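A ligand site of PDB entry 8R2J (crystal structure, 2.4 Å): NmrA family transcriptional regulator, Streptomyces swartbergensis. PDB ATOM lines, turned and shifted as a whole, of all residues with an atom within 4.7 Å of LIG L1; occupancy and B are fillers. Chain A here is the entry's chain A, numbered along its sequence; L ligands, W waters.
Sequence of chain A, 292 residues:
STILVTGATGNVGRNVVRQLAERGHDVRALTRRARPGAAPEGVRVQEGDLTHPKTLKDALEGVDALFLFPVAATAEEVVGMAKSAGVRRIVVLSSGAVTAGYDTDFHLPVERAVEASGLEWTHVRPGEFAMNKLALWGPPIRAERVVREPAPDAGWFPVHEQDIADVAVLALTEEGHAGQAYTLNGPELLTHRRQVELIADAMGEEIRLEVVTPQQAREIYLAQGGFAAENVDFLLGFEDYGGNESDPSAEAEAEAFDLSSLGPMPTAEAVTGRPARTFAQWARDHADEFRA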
ATOM      1  N   GLY A   7      -4.812  29.142  13.149  1.00  0.00           N
ATOM      2  CA  GLY A   7      -6.107  28.889  12.476  1.00  0.00           C
ATOM      3  C   GLY A   7      -6.786  30.178  12.024  1.00  0.00           C
ATOM      4  O   GLY A   7      -8.001  30.130  11.791  1.00  0.00           O
ATOM      5  N   ALA A   8      -6.008  31.253  11.822  1.00  0.00           N
ATOM      6  CA  ALA A   8      -6.440  32.644  11.539  1.00  0.00           C
ATOM      7  C   ALA A   8      -7.186  32.785  10.217  1.00  0.00           C
ATOM      8  O   ALA A   8      -8.000  33.682  10.181  1.00  0.00           O
ATOM      9  CB  ALA A   8      -5.260  33.574  11.511  1.00  0.00           C
ATOM     10  N   THR A   9      -6.827  32.051   9.163  1.00  0.00           N
ATOM     11  CA  THR A   9      -7.505  32.097   7.844  1.00  0.00           C
ATOM     12  C   THR A   9      -8.709  31.148   7.844  1.00  0.00           C
ATOM     13  O   THR A   9      -9.434  31.148   6.847  1.00  0.00           O
ATOM     14  CB  THR A   9      -6.537  31.758   6.721  1.00  0.00           C
ATOM     15  OG1 THR A   9      -6.020  30.450   6.924  1.00  0.00           O
ATOM     16  CG2 THR A   9      -5.402  32.765   6.644  1.00  0.00           C
ATOM     17  N   GLY A  10      -8.961  30.436   8.932  1.00  0.00           N
ATOM     18  CA  GLY A  10     -10.021  29.413   8.994  1.00  0.00           C
ATOM     19  C   GLY A  10     -11.389  30.001   9.315  1.00  0.00           C
ATOM     20  O   GLY A  10     -11.498  31.182   9.782  1.00  0.00           O
ATOM     21  N   ASN A  11     -12.412  29.166   9.110  1.00  0.00           N
ATOM     22  CA  ASN A  11     -13.831  29.494   9.367  1.00  0.00           C
ATOM     23  C   ASN A  11     -13.951  30.174  10.734  1.00  0.00           C
ATOM     24  O   ASN A  11     -14.633  31.194  10.833  1.00  0.00           O
ATOM     25  CB  ASN A  11     -14.702  28.242   9.273  1.00  0.00           C
ATOM     26  CG  ASN A  11     -14.737  27.712   7.864  1.00  0.00           C
ATOM     27  OD1 ASN A  11     -14.925  28.497   6.939  1.00  0.00           O
ATOM     28  ND2 ASN A  11     -14.482  26.418   7.698  1.00  0.00           N
ATOM     29  N   VAL A  12     -13.313  29.631  11.759  1.00  0.00           N
ATOM     30  CA  VAL A  12     -13.430  30.132  13.147  1.00  0.00           C
ATOM     31  C   VAL A  12     -12.435  31.259  13.331  1.00  0.00           C
ATOM     32  O   VAL A  12     -12.886  32.360  13.653  1.00  0.00           O
ATOM     33  CB  VAL A  12     -13.204  28.996  14.155  1.00  0.00           C
ATOM     34  CG1 VAL A  12     -13.231  29.514  15.569  1.00  0.00           C
ATOM     35  CG2 VAL A  12     -14.232  27.891  13.935  1.00  0.00           C
ATOM     36  N   GLY A  13     -11.160  31.022  13.056  1.00  0.00           N
ATOM     37  CA  GLY A  13     -10.090  32.018  13.276  1.00  0.00           C
ATOM     38  C   GLY A  13     -10.306  33.364  12.555  1.00  0.00           C
ATOM     39  O   GLY A  13      -9.932  34.387  13.189  1.00  0.00           O
ATOM     40  N   LEU A  30      -1.295  33.780  12.424  1.00  0.00           N
ATOM     41  CA  LEU A  30      -0.399  32.719  11.910  1.00  0.00           C
ATOM     42  C   LEU A  30      -1.044  32.029  10.709  1.00  0.00           C
ATOM     43  O   LEU A  30      -2.212  31.556  10.831  1.00  0.00           O
ATOM     44  CB  LEU A  30      -0.112  31.662  12.988  1.00  0.00           C
ATOM     45  CG  LEU A  30       0.984  30.684  12.594  1.00  0.00           C
ATOM     46  CD1 LEU A  30       2.355  31.308  12.846  1.00  0.00           C
ATOM     47  CD2 LEU A  30       0.853  29.375  13.351  1.00  0.00           C
ATOM     48  N   THR A  31      -0.288  31.974   9.604  1.00  0.00           N
ATOM     49  CA  THR A  31      -0.611  31.224   8.389  1.00  0.00           C
ATOM     50  C   THR A  31       0.673  30.586   7.845  1.00  0.00           C
ATOM     51  O   THR A  31       1.783  31.168   8.021  1.00  0.00           O
ATOM     52  CB  THR A  31      -1.312  32.133   7.377  1.00  0.00           C
ATOM     53  OG1 THR A  31      -1.573  31.425   6.159  1.00  0.00           O
ATOM     54  CG2 THR A  31      -0.478  33.342   6.987  1.00  0.00           C
ATOM     55  N   ARG A  32       0.536  29.472   7.137  1.00  0.00           N
ATOM     56  CA  ARG A  32       1.674  28.825   6.451  1.00  0.00           C
ATOM     57  C   ARG A  32       2.117  29.664   5.245  1.00  0.00           C
ATOM     58  O   ARG A  32       3.295  29.556   4.912  1.00  0.00           O
ATOM     59  CB  ARG A  32       1.326  27.389   6.073  1.00  0.00           C
ATOM     60  CG  ARG A  32       1.249  26.525   7.314  1.00  0.00           C
ATOM     61  CD  ARG A  32       0.547  25.215   7.054  1.00  0.00           C
ATOM     62  NE  ARG A  32      -0.874  25.335   6.741  1.00  0.00           N
ATOM     63  CZ  ARG A  32      -1.645  24.296   6.432  1.00  0.00           C
ATOM     64  NH1 ARG A  32      -1.169  23.070   6.403  1.00  0.00           N
ATOM     65  NH2 ARG A  32      -2.921  24.468   6.185  1.00  0.00           N
ATOM     66  N   ARG A  33       1.256  30.475   4.636  1.00  0.00           N
ATOM     67  CA  ARG A  33       1.719  31.337   3.519  1.00  0.00           C
ATOM     68  C   ARG A  33       1.205  32.744   3.752  1.00  0.00           C
ATOM     69  O   ARG A  33       0.002  32.971   3.589  1.00  0.00           O
ATOM     70  CB  ARG A  33       1.275  30.797   2.162  1.00  0.00           C
ATOM     71  CG  ARG A  33       2.326  30.900   1.059  1.00  0.00           C
ATOM     72  CD  ARG A  33       1.758  30.573  -0.321  1.00  0.00           C
ATOM     73  NE  ARG A  33       0.614  31.463  -0.583  1.00  0.00           N
ATOM     74  CZ  ARG A  33      -0.688  31.132  -0.670  1.00  0.00           C
ATOM     75  NH1 ARG A  33      -1.100  29.877  -0.575  1.00  0.00           N
ATOM     76  NH2 ARG A  33      -1.583  32.088  -0.871  1.00  0.00           N
ATOM     77  N   ARG A  35       0.322  36.335   3.050  1.00  0.00           N
ATOM     78  CA  ARG A  35      -0.120  37.169   1.909  1.00  0.00           C
ATOM     79  C   ARG A  35      -1.104  38.194   2.450  1.00  0.00           C
ATOM     80  O   ARG A  35      -1.673  38.003   3.526  1.00  0.00           O
ATOM     81  CB  ARG A  35      -0.725  36.276   0.824  1.00  0.00           C
ATOM     82  CG  ARG A  35      -2.203  35.981   1.022  1.00  0.00           C
ATOM     83  CD  ARG A  35      -2.490  34.519   1.305  1.00  0.00           C
ATOM     84  NE  ARG A  35      -3.850  34.323   1.788  1.00  0.00           N
ATOM     85  CZ  ARG A  35      -4.242  33.387   2.646  1.00  0.00           C
ATOM     86  NH1 ARG A  35      -3.362  32.532   3.173  1.00  0.00           N
ATOM     87  NH2 ARG A  35      -5.531  33.305   2.963  1.00  0.00           N
ATOM     88  N   GLY A  48       4.382  30.743   9.457  1.00  0.00           N
ATOM     89  CA  GLY A  48       4.806  29.646  10.346  1.00  0.00           C
ATOM     90  C   GLY A  48       3.957  28.414  10.183  1.00  0.00           C
ATOM     91  O   GLY A  48       2.913  28.484   9.568  1.00  0.00           O
ATOM     92  N   ASP A  49       4.421  27.298  10.729  1.00  0.00           N
ATOM     93  CA  ASP A  49       3.798  25.970  10.513  1.00  0.00           C
ATOM     94  C   ASP A  49       3.802  25.272  11.868  1.00  0.00           C
ATOM     95  O   ASP A  49       4.861  25.118  12.454  1.00  0.00           O
ATOM     96  CB  ASP A  49       4.491  25.161   9.395  1.00  0.00           C
ATOM     97  CG  ASP A  49       3.636  23.977   8.906  1.00  0.00           C
ATOM     98  OD1 ASP A  49       3.053  23.289   9.770  1.00  0.00           O
ATOM     99  OD2 ASP A  49       3.567  23.746   7.658  1.00  0.00           O
ATOM    100  N   LEU A  50       2.621  24.887  12.319  1.00  0.00           N
ATOM    101  CA  LEU A  50       2.430  24.182  13.586  1.00  0.00           C
ATOM    102  C   LEU A  50       3.166  22.854  13.547  1.00  0.00           C
ATOM    103  O   LEU A  50       3.537  22.405  14.625  1.00  0.00           O
ATOM    104  CB  LEU A  50       0.930  23.973  13.829  1.00  0.00           C
ATOM    105  CG  LEU A  50       0.226  25.243  14.303  1.00  0.00           C
ATOM    106  CD1 LEU A  50      -1.272  25.116  14.155  1.00  0.00           C
ATOM    107  CD2 LEU A  50       0.625  25.570  15.747  1.00  0.00           C
ATOM    108  N   THR A  51       3.379  22.243  12.380  1.00  0.00           N
ATOM    109  CA  THR A  51       4.092  20.922  12.291  1.00  0.00           C
ATOM    110  C   THR A  51       5.611  21.104  12.360  1.00  0.00           C
ATOM    111  O   THR A  51       6.294  20.086  12.478  1.00  0.00           O
ATOM    112  CB  THR A  51       3.664  20.117  11.060  1.00  0.00           C
ATOM    113  OG1 THR A  51       4.036  20.839   9.899  1.00  0.00           O
ATOM    114  CG2 THR A  51       2.177  19.862  11.033  1.00  0.00           C
ATOM    115  N   PHE A  69      -4.904  26.202  17.147  1.00  0.00           N
ATOM    116  CA  PHE A  69      -5.508  25.252  16.177  1.00  0.00           C
ATOM    117  C   PHE A  69      -4.938  23.872  16.482  1.00  0.00           C
ATOM    118  O   PHE A  69      -3.768  23.753  16.809  1.00  0.00           O
ATOM    119  CB  PHE A  69      -5.207  25.692  14.728  1.00  0.00           C
ATOM    120  CG  PHE A  69      -5.970  24.910  13.700  1.00  0.00           C
ATOM    121  CD1 PHE A  69      -7.291  25.218  13.411  1.00  0.00           C
ATOM    122  CD2 PHE A  69      -5.415  23.771  13.124  1.00  0.00           C
ATOM    123  CE1 PHE A  69      -8.037  24.429  12.543  1.00  0.00           C
ATOM    124  CE2 PHE A  69      -6.144  22.995  12.231  1.00  0.00           C
ATOM    125  CZ  PHE A  69      -7.459  23.327  11.942  1.00  0.00           C
ATOM    126  N   PRO A  70      -5.736  22.797  16.491  1.00  0.00           N
ATOM    127  CA  PRO A  70      -5.226  21.492  16.964  1.00  0.00           C
ATOM    128  C   PRO A  70      -4.303  20.696  16.032  1.00  0.00           C
ATOM    129  O   PRO A  70      -4.697  20.300  14.923  1.00  0.00           O
ATOM    130  CB  PRO A  70      -6.499  20.665  17.194  1.00  0.00           C
ATOM    131  CG  PRO A  70      -7.538  21.310  16.287  1.00  0.00           C
ATOM    132  CD  PRO A  70      -7.178  22.787  16.246  1.00  0.00           C
ATOM    133  N   VAL A  71      -3.083  20.456  16.503  1.00  0.00           N
ATOM    134  CA  VAL A  71      -2.118  19.582  15.790  1.00  0.00           C
ATOM    135  C   VAL A  71      -1.415  18.736  16.854  1.00  0.00           C
ATOM    136  O   VAL A  71      -0.383  19.178  17.462  1.00  0.00           O
ATOM    137  CB  VAL A  71      -1.202  20.412  14.875  1.00  0.00           C
ATOM    138  CG1 VAL A  71      -0.177  19.560  14.168  1.00  0.00           C
ATOM    139  CG2 VAL A  71      -2.010  21.215  13.852  1.00  0.00           C
ATOM    140  N   LEU A  93      -8.877  25.264  20.084  1.00  0.00           N
ATOM    141  CA  LEU A  93      -9.970  24.788  19.197  1.00  0.00           C
ATOM    142  C   LEU A  93      -9.988  23.257  19.272  1.00  0.00           C
ATOM    143  O   LEU A  93      -9.119  22.625  18.679  1.00  0.00           O
ATOM    144  CB  LEU A  93      -9.785  25.289  17.772  1.00  0.00           C
ATOM    145  CG  LEU A  93     -10.825  24.792  16.764  1.00  0.00           C
ATOM    146  CD1 LEU A  93     -12.241  25.053  17.259  1.00  0.00           C
ATOM    147  CD2 LEU A  93     -10.649  25.498  15.445  1.00  0.00           C
ATOM    148  N   SER A  94     -10.917  22.700  20.054  1.00  0.00           N
ATOM    149  CA  SER A  94     -11.008  21.247  20.291  1.00  0.00           C
ATOM    150  C   SER A  94     -12.272  20.753  19.596  1.00  0.00           C
ATOM    151  O   SER A  94     -12.563  21.201  18.470  1.00  0.00           O
ATOM    152  CB  SER A  94     -10.975  20.926  21.757  1.00  0.00           C
ATOM    153  OG  SER A  94     -11.092  19.519  21.958  1.00  0.00           O
ATOM    154  N   SER A  95     -12.992  19.826  20.234  1.00  0.00           N
ATOM    155  CA  SER A  95     -14.108  19.112  19.573  1.00  0.00           C
ATOM    156  C   SER A  95     -15.039  18.526  20.644  1.00  0.00           C
ATOM    157  O   SER A  95     -14.514  18.009  21.667  1.00  0.00           O
ATOM    158  CB  SER A  95     -13.560  18.072  18.702  1.00  0.00           C
ATOM    159  OG  SER A  95     -14.584  17.275  18.220  1.00  0.00           O
ATOM    160  N   PHE A 106      -7.008  12.584  19.045  1.00  0.00           N
ATOM    161  CA  PHE A 106      -6.674  13.733  18.163  1.00  0.00           C
ATOM    162  C   PHE A 106      -6.798  15.054  18.894  1.00  0.00           C
ATOM    163  O   PHE A 106      -5.803  15.771  19.022  1.00  0.00           O
ATOM    164  CB  PHE A 106      -7.498  13.814  16.882  1.00  0.00           C
ATOM    165  CG  PHE A 106      -6.961  14.923  16.025  1.00  0.00           C
ATOM    166  CD1 PHE A 106      -5.659  14.880  15.524  1.00  0.00           C
ATOM    167  CD2 PHE A 106      -7.726  16.067  15.817  1.00  0.00           C
ATOM    168  CE1 PHE A 106      -5.131  15.947  14.796  1.00  0.00           C
ATOM    169  CE2 PHE A 106      -7.213  17.121  15.078  1.00  0.00           C
ATOM    170  CZ  PHE A 106      -5.910  17.074  14.590  1.00  0.00           C
ATOM    171  N   HIS A 107      -7.987  15.431  19.326  1.00  0.00           N
ATOM    172  CA  HIS A 107      -8.145  16.719  20.040  1.00  0.00           C
ATOM    173  C   HIS A 107      -7.711  16.545  21.486  1.00  0.00           C
ATOM    174  O   HIS A 107      -7.190  17.515  22.001  1.00  0.00           O
ATOM    175  CB  HIS A 107      -9.551  17.265  19.915  1.00  0.00           C
ATOM    176  CG  HIS A 107      -9.887  17.679  18.525  1.00  0.00           C
ATOM    177  ND1 HIS A 107     -10.558  16.848  17.664  1.00  0.00           N
ATOM    178  CD2 HIS A 107      -9.647  18.824  17.867  1.00  0.00           C
ATOM    179  CE1 HIS A 107     -10.698  17.470  16.511  1.00  0.00           C
ATOM    180  NE2 HIS A 107     -10.136  18.677  16.598  1.00  0.00           N
ATOM    181  N   PRO A 126     -16.564  22.602  19.845  1.00  0.00           N
ATOM    182  CA  PRO A 126     -17.701  22.647  18.955  1.00  0.00           C
ATOM    183  C   PRO A 126     -18.163  21.229  18.638  1.00  0.00           C
ATOM    184  O   PRO A 126     -17.334  20.321  18.536  1.00  0.00           O
ATOM    185  CB  PRO A 126     -17.207  23.277  17.655  1.00  0.00           C
ATOM    186  CG  PRO A 126     -15.715  23.254  17.761  1.00  0.00           C
ATOM    187  CD  PRO A 126     -15.398  23.248  19.243  1.00  0.00           C
ATOM    188  N   GLY A 127     -19.468  21.081  18.516  1.00  0.00           N
ATOM    189  CA  GLY A 127     -20.063  19.908  17.881  1.00  0.00           C
ATOM    190  C   GLY A 127     -19.976  20.023  16.366  1.00  0.00           C
ATOM    191  O   GLY A 127     -19.036  20.700  15.862  1.00  0.00           O
ATOM    192  N   GLU A 128     -20.929  19.408  15.659  1.00  0.00           N
ATOM    193  CA  GLU A 128     -21.003  19.415  14.178  1.00  0.00           C
ATOM    194  C   GLU A 128     -21.068  20.835  13.658  1.00  0.00           C
ATOM    195  O   GLU A 128     -22.047  21.473  13.926  1.00  0.00           O
ATOM    196  CB  GLU A 128     -22.293  18.742  13.714  1.00  0.00           C
ATOM    197  CG  GLU A 128     -22.299  18.502  12.216  1.00  0.00           C
ATOM    198  CD  GLU A 128     -23.684  18.157  11.723  1.00  0.00           C
ATOM    199  OE1 GLU A 128     -24.668  18.536  12.419  1.00  0.00           O
ATOM    200  OE2 GLU A 128     -23.771  17.479  10.683  1.00  0.00           O
ATOM    201  N   PHE A 129     -20.107  21.248  12.855  1.00  0.00           N
ATOM    202  CA  PHE A 129     -20.129  22.548  12.144  1.00  0.00           C
ATOM    203  C   PHE A 129     -21.249  22.573  11.106  1.00  0.00           C
ATOM    204  O   PHE A 129     -21.374  21.649  10.267  1.00  0.00           O
ATOM    205  CB  PHE A 129     -18.830  22.815  11.397  1.00  0.00           C
ATOM    206  CG  PHE A 129     -17.650  23.259  12.219  1.00  0.00           C
ATOM    207  CD1 PHE A 129     -17.413  22.760  13.478  1.00  0.00           C
ATOM    208  CD2 PHE A 129     -16.731  24.151  11.669  1.00  0.00           C
ATOM    209  CE1 PHE A 129     -16.294  23.155  14.196  1.00  0.00           C
ATOM    210  CE2 PHE A 129     -15.607  24.552  12.381  1.00  0.00           C
ATOM    211  CZ  PHE A 129     -15.394  24.052  13.655  1.00  0.00           C
ATOM    212  N   ASN A 132     -20.088  22.163   7.536  1.00  0.00           N
ATOM    213  CA  ASN A 132     -20.071  20.810   6.938  1.00  0.00           C
ATOM    214  C   ASN A 132     -21.131  20.773   5.824  1.00  0.00           C
ATOM    215  O   ASN A 132     -20.931  20.039   4.864  1.00  0.00           O
ATOM    216  CB  ASN A 132     -20.226  19.703   7.980  1.00  0.00           C
ATOM    217  CG  ASN A 132     -19.069  19.605   8.948  1.00  0.00           C
ATOM    218  OD1 ASN A 132     -18.090  20.313   8.834  1.00  0.00           O
ATOM    219  ND2 ASN A 132     -19.155  18.709   9.902  1.00  0.00           N
HETATM  220  P1  LIG L   1     -10.521  25.685   8.467  1.00  0.00           P
HETATM  221  O1  LIG L   1     -11.007  27.002   7.952  1.00  0.00           O
HETATM  222  O2  LIG L   1     -10.943  24.414   7.788  1.00  0.00           O
HETATM  223  O3  LIG L   1      -8.969  25.546   8.733  1.00  0.00           O
HETATM  224  C1  LIG L   1      -8.012  26.409   8.254  1.00  0.00           C
HETATM  225  C2  LIG L   1      -7.072  26.887   9.340  1.00  0.00           C
HETATM  226  O4  LIG L   1      -6.175  25.933   9.975  1.00  0.00           O
HETATM  227  C3  LIG L   1      -6.182  27.811   8.518  1.00  0.00           C
HETATM  228  O5  LIG L   1      -6.096  29.058   9.174  1.00  0.00           O
HETATM  229  C4  LIG L   1      -4.874  27.058   8.456  1.00  0.00           C
HETATM  230  O6  LIG L   1      -3.826  27.939   8.220  1.00  0.00           O
HETATM  231  C5  LIG L   1      -4.826  26.424   9.823  1.00  0.00           C
HETATM  232  N1  LIG L   1      -3.797  25.370   9.809  1.00  0.00           N
HETATM  233  C6  LIG L   1      -4.010  24.082   9.507  1.00  0.00           C
HETATM  234  N2  LIG L   1      -2.859  23.382   9.617  1.00  0.00           N
HETATM  235  C7  LIG L   1      -1.902  24.242   9.973  1.00  0.00           C
HETATM  236  C8  LIG L   1      -0.466  24.149  10.220  1.00  0.00           C
HETATM  237  N3  LIG L   1       0.141  22.964  10.112  1.00  0.00           N
HETATM  238  N4  LIG L   1       0.200  25.246  10.596  1.00  0.00           N
HETATM  239  C9  LIG L   1      -0.440  26.419  10.715  1.00  0.00           C
HETATM  240  N5  LIG L   1      -1.756  26.585  10.482  1.00  0.00           N
HETATM  241  C10 LIG L   1      -2.519  25.549  10.107  1.00  0.00           C
HETATM  242  O7  LIG L   1     -10.645  25.567  10.042  1.00  0.00           O
HETATM  243  P2  LIG L   1     -11.951  25.818  10.875  1.00  0.00           P
HETATM  244  O8  LIG L   1     -13.128  25.206  10.130  1.00  0.00           O
HETATM  245  O9  LIG L   1     -11.780  27.217  11.394  1.00  0.00           O
HETATM  246  O10 LIG L   1     -11.554  24.764  11.995  1.00  0.00           O
HETATM  247  C11 LIG L   1     -11.793  23.397  11.735  1.00  0.00           C
HETATM  248  C12 LIG L   1     -11.338  22.618  12.947  1.00  0.00           C
HETATM  249  O11 LIG L   1     -12.391  22.606  13.924  1.00  0.00           O
HETATM  250  C13 LIG L   1     -11.065  21.152  12.611  1.00  0.00           C
HETATM  251  O12 LIG L   1      -9.744  20.909  12.153  1.00  0.00           O
HETATM  252  C14 LIG L   1     -11.344  20.483  13.930  1.00  0.00           C
HETATM  253  O13 LIG L   1     -10.156  20.476  14.704  1.00  0.00           O
HETATM  254  C15 LIG L   1     -12.376  21.367  14.618  1.00  0.00           C
HETATM  255  N6  LIG L   1     -13.691  20.738  14.602  1.00  0.00           N
HETATM  256  C16 LIG L   1     -14.427  20.602  13.463  1.00  0.00           C
HETATM  257  C17 LIG L   1     -15.696  19.972  13.468  1.00  0.00           C
HETATM  258  C18 LIG L   1     -16.564  19.846  12.222  1.00  0.00           C
HETATM  259  O14 LIG L   1     -17.757  19.520  12.298  1.00  0.00           O
HETATM  260  N7  LIG L   1     -16.059  20.137  11.017  1.00  0.00           N
HETATM  261  C19 LIG L   1     -16.200  19.516  14.655  1.00  0.00           C
HETATM  262  C20 LIG L   1     -15.433  19.672  15.794  1.00  0.00           C
HETATM  263  C21 LIG L   1     -14.176  20.280  15.766  1.00  0.00           C
HETATM  264  P3  LIG L   1      -3.280  28.197   6.711  1.00  0.00           P
HETATM  265  O15 LIG L   1      -3.545  29.661   6.427  1.00  0.00           O
HETATM  266  O16 LIG L   1      -1.822  27.919   6.970  1.00  0.00           O
HETATM  267  O17 LIG L   1      -4.009  27.230   5.821  1.00  0.00           O
HETATM  268  C1  LG2 L   2     -20.958  15.422  13.661  1.00  0.00           C
HETATM  269  C2  LG2 L   2     -21.627  15.333  14.871  1.00  0.00           C
HETATM  270  C3  LG2 L   2     -20.957  15.562  16.066  1.00  0.00           C
HETATM  271  C4  LG2 L   2     -19.573  15.838  16.051  1.00  0.00           C
HETATM  272  O1  LG2 L   2     -18.862  16.057  17.189  1.00  0.00           O
HETATM  273  C5  LG2 L   2     -18.848  15.915  14.835  1.00  0.00           C
HETATM  274  C6  LG2 L   2     -17.357  16.200  14.790  1.00  0.00           C
HETATM  275  O2  LG2 L   2     -16.739  16.323  15.847  1.00  0.00           O
HETATM  276  C7  LG2 L   2     -16.637  16.331  13.451  1.00  0.00           C
HETATM  277  C8  LG2 L   2     -15.223  16.660  13.304  1.00  0.00           C
HETATM  278  O3  LG2 L   2     -14.465  16.852  14.447  1.00  0.00           O
HETATM  279  C9  LG2 L   2     -14.596  16.770  12.027  1.00  0.00           C
HETATM  280  C10 LG2 L   2     -13.145  17.167  11.677  1.00  0.00           C
HETATM  281  O4  LG2 L   2     -12.133  17.019  12.700  1.00  0.00           O
HETATM  282  C11 LG2 L   2     -12.646  16.400  10.467  1.00  0.00           C
HETATM  283  C12 LG2 L   2     -13.421  16.714   9.188  1.00  0.00           C
HETATM  284  O5  LG2 L   2     -12.985  15.823   8.116  1.00  0.00           O
HETATM  285  C13 LG2 L   2     -13.054  18.083   8.551  1.00  0.00           C
HETATM  286  O6  LG2 L   2     -13.907  18.888   8.290  1.00  0.00           O
HETATM  287  C14 LG2 L   2     -11.606  18.337   8.191  1.00  0.00           C
HETATM  288  O7  LG2 L   2     -10.800  18.810   9.248  1.00  0.00           O
HETATM  289  C15 LG2 L   2     -14.932  16.627   9.457  1.00  0.00           C
HETATM  290  C16 LG2 L   2     -15.418  16.544  10.896  1.00  0.00           C
HETATM  291  C17 LG2 L   2     -16.770  16.228  11.039  1.00  0.00           C
HETATM  292  O8  LG2 L   2     -17.503  16.023   9.921  1.00  0.00           O
HETATM  293  C18 LG2 L   2     -17.404  16.103  12.289  1.00  0.00           C
HETATM  294  C19 LG2 L   2     -18.880  15.751  12.348  1.00  0.00           C
HETATM  295  O9  LG2 L   2     -19.527  15.483  11.333  1.00  0.00           O
HETATM  296  C20 LG2 L   2     -19.581  15.703  13.647  1.00  0.00           C
HETATM  297  C21 LG2 L   2     -19.614  16.288  18.390  1.00  0.00           C
HETATM  298  C22 LG2 L   2     -10.827  16.472  12.462  1.00  0.00           C
HETATM  299  C23 LG2 L   2     -10.902  14.957  12.312  1.00  0.00           C
HETATM  300  C24 LG2 L   2     -10.660  14.404  10.903  1.00  0.00           C
HETATM  301  N1  LG2 L   2     -10.465  12.955  10.970  1.00  0.00           N
HETATM  302  C25 LG2 L   2      -9.478  15.081  10.184  1.00  0.00           C
HETATM  303  O10 LG2 L   2      -8.375  14.194  10.083  1.00  0.00           O
HETATM  304  C26 LG2 L   2      -9.017  16.333  10.908  1.00  0.00           C
HETATM  305  O11 LG2 L   2     -10.172  17.080  11.352  1.00  0.00           O
HETATM  306  C27 LG2 L   2      -8.178  16.010  12.115  1.00  0.00           C
HETATM  307  O   HOH W   1     -11.205  27.890   5.271  1.00  0.00           O
HETATM  308  O   HOH W   2      -2.310  29.022  11.869  1.00  0.00           O
HETATM  309  O   HOH W   3     -14.298  23.145   8.972  1.00  0.00           O
HETATM  310  O   HOH W   4      -6.184  21.836   8.520  1.00  0.00           O
HETATM  311  O   HOH W   5      -1.095  20.321   9.416  1.00  0.00           O
HETATM  312  O   HOH W   6     -13.404  20.708   9.995  1.00  0.00           O
HETATM  313  O   HOH W   7      -6.301  26.775   4.910  1.00  0.00           O
HETATM  314  O   HOH W   8      -9.876  28.465  12.753  1.00  0.00           O
HETATM  315  O   HOH W   9      -4.180  30.613   9.300  1.00  0.00           O
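An oxygen (O5) of LIG L1 is in hydrogen-bond range of the backbone NH (N) of Ala 8, at 3.4 Å.
NE2 of His 107 lies within hydrogen-bond range of O13 of LIG L1, 2.6 Å away.
NE of Arg 32 lies within salt-bridge range of O16 of LIG L1 (2.8 Å).
O15 of LIG L1 lies within hydrogen-bond range of OG1 of Thr 9 (2.6 Å).
An oxygen (O8) of LG2 L2 is in hydrogen-bond range of the side-chain amide nitrogen (ND2) of Asn 132 (3.2 Å).
N of Arg 32 lies within hydrogen-bond range of O16 of LIG L1.
N of Gly 10 lies within hydrogen-bond range of O5 of LIG L1, at 3.2 Å.
An oxygen (O1) of LIG L1 is in hydrogen-bond range of the backbone NH of Asn 11 (2.8 Å).
The backbone carbonyl oxygen of Gly 7 sits close to an oxygen (O5) of LIG L1.
The side-chain amide nitrogen (ND2) of Asn 11 is in hydrogen-bond range of an oxygen (O8) of LIG L1 (3.0 Å).
O14 of LIG L1 sits at hydrogen-bond distance from ND2 of Asn 132 (2.9 Å).
The side-chain hydroxyl of Ser 95 sits at hydrogen-bond distance from an oxygen (O2) of LG2 L2 (3.3 Å).
N of Val 12 sits at hydrogen-bond distance from O9 of LIG L1.
An oxygen (O14) of LIG L1 is in hydrogen-bond range of the backbone NH (N) of Phe 129 (3.0 Å).
The backbone NH of Leu 50 sits at hydrogen-bond distance from a nitrogen (N4) of LIG L1, at 3.0 Å.
N of Thr 9 is in hydrogen-bond range of O5 of LIG L1 (3.1 Å).
An oxygen (O15) of LIG L1 is in hydrogen-bond range of the side-chain hydroxyl (OG1) of Thr 31, 2.7 Å away.
The side-chain carboxylate (OD1) of Asp 49 sits at hydrogen-bond distance from a nitrogen (N3) of LIG L1 (2.9 Å).
O of Thr 31 lies within hydrogen-bond range of N of Gly 48, 3.0 Å away.
The side-chain hydroxyl (OG1) of Thr 31 lies close to the backbone NH (N) of Arg 33 (3.4 Å).
The side-chain carboxylate of Asp 49 lies within hydrogen-bond range of the side-chain hydroxyl of Thr 51 (2.6 Å).
Residues that only touch LIG L1: Pro 70 (3.2 Å), Ser 94 (3.3 Å), Gly 127 (3.3 Å), Phe 69 (3.3 Å), Pro 126 (3.4 Å), Ser 95 (3.5 Å), Leu 93 (3.6 Å), Glu 128 (3.8 Å) and Thr 51 (3.8 Å).
Hydrophobic or aromatic side chains that line LIG L1: Val 12, Leu 50, Phe 69, Pro 70, Leu 93, His 107, Pro 126 and Phe 129.
Within 4 Å of LIG L1: Gly 7, Ala 8, Thr 9, Gly 10, Asn 11, Val 12, Thr 31, Arg 32, Asp 49, Leu 50, Thr 51, Phe 69, Pro 70, Leu 93, Ser 94, Ser 95, His 107, Pro 126, Gly 127, Glu 128, Phe 129 and Asn 132.
The nearest printed residue that does not touch LIG L1 is Gly 48 (4.1 Å).
Water W9 lies within hydrogen-bond range of an oxygen (O5) of LIG L1 (2.5 Å), the backbone carbonyl oxygen of Leu 30 (2.7 Å), the side-chain hydroxyl of Thr 9 (3.0 Å) and the backbone NH of Ala 8 (3.2 Å).
Water W8 lies within hydrogen-bond range of O9 of LIG L1 (2.7 Å), O of Gly 7 (2.7 Å) and N of Gly 13 (2.9 Å).
Water W2 lies within hydrogen-bond range of the backbone carbonyl oxygen (O) of Leu 30 (2.7 Å), the backbone NH (N) of Gly 7 (2.8 Å) and a nitrogen (N5) of LIG L1 (2.9 Å).
Water W6 lies within hydrogen-bond range of an oxygen (O6) of LG2 L2 (2.5 Å) and a nitrogen (N7) of LIG L1 (2.9 Å).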
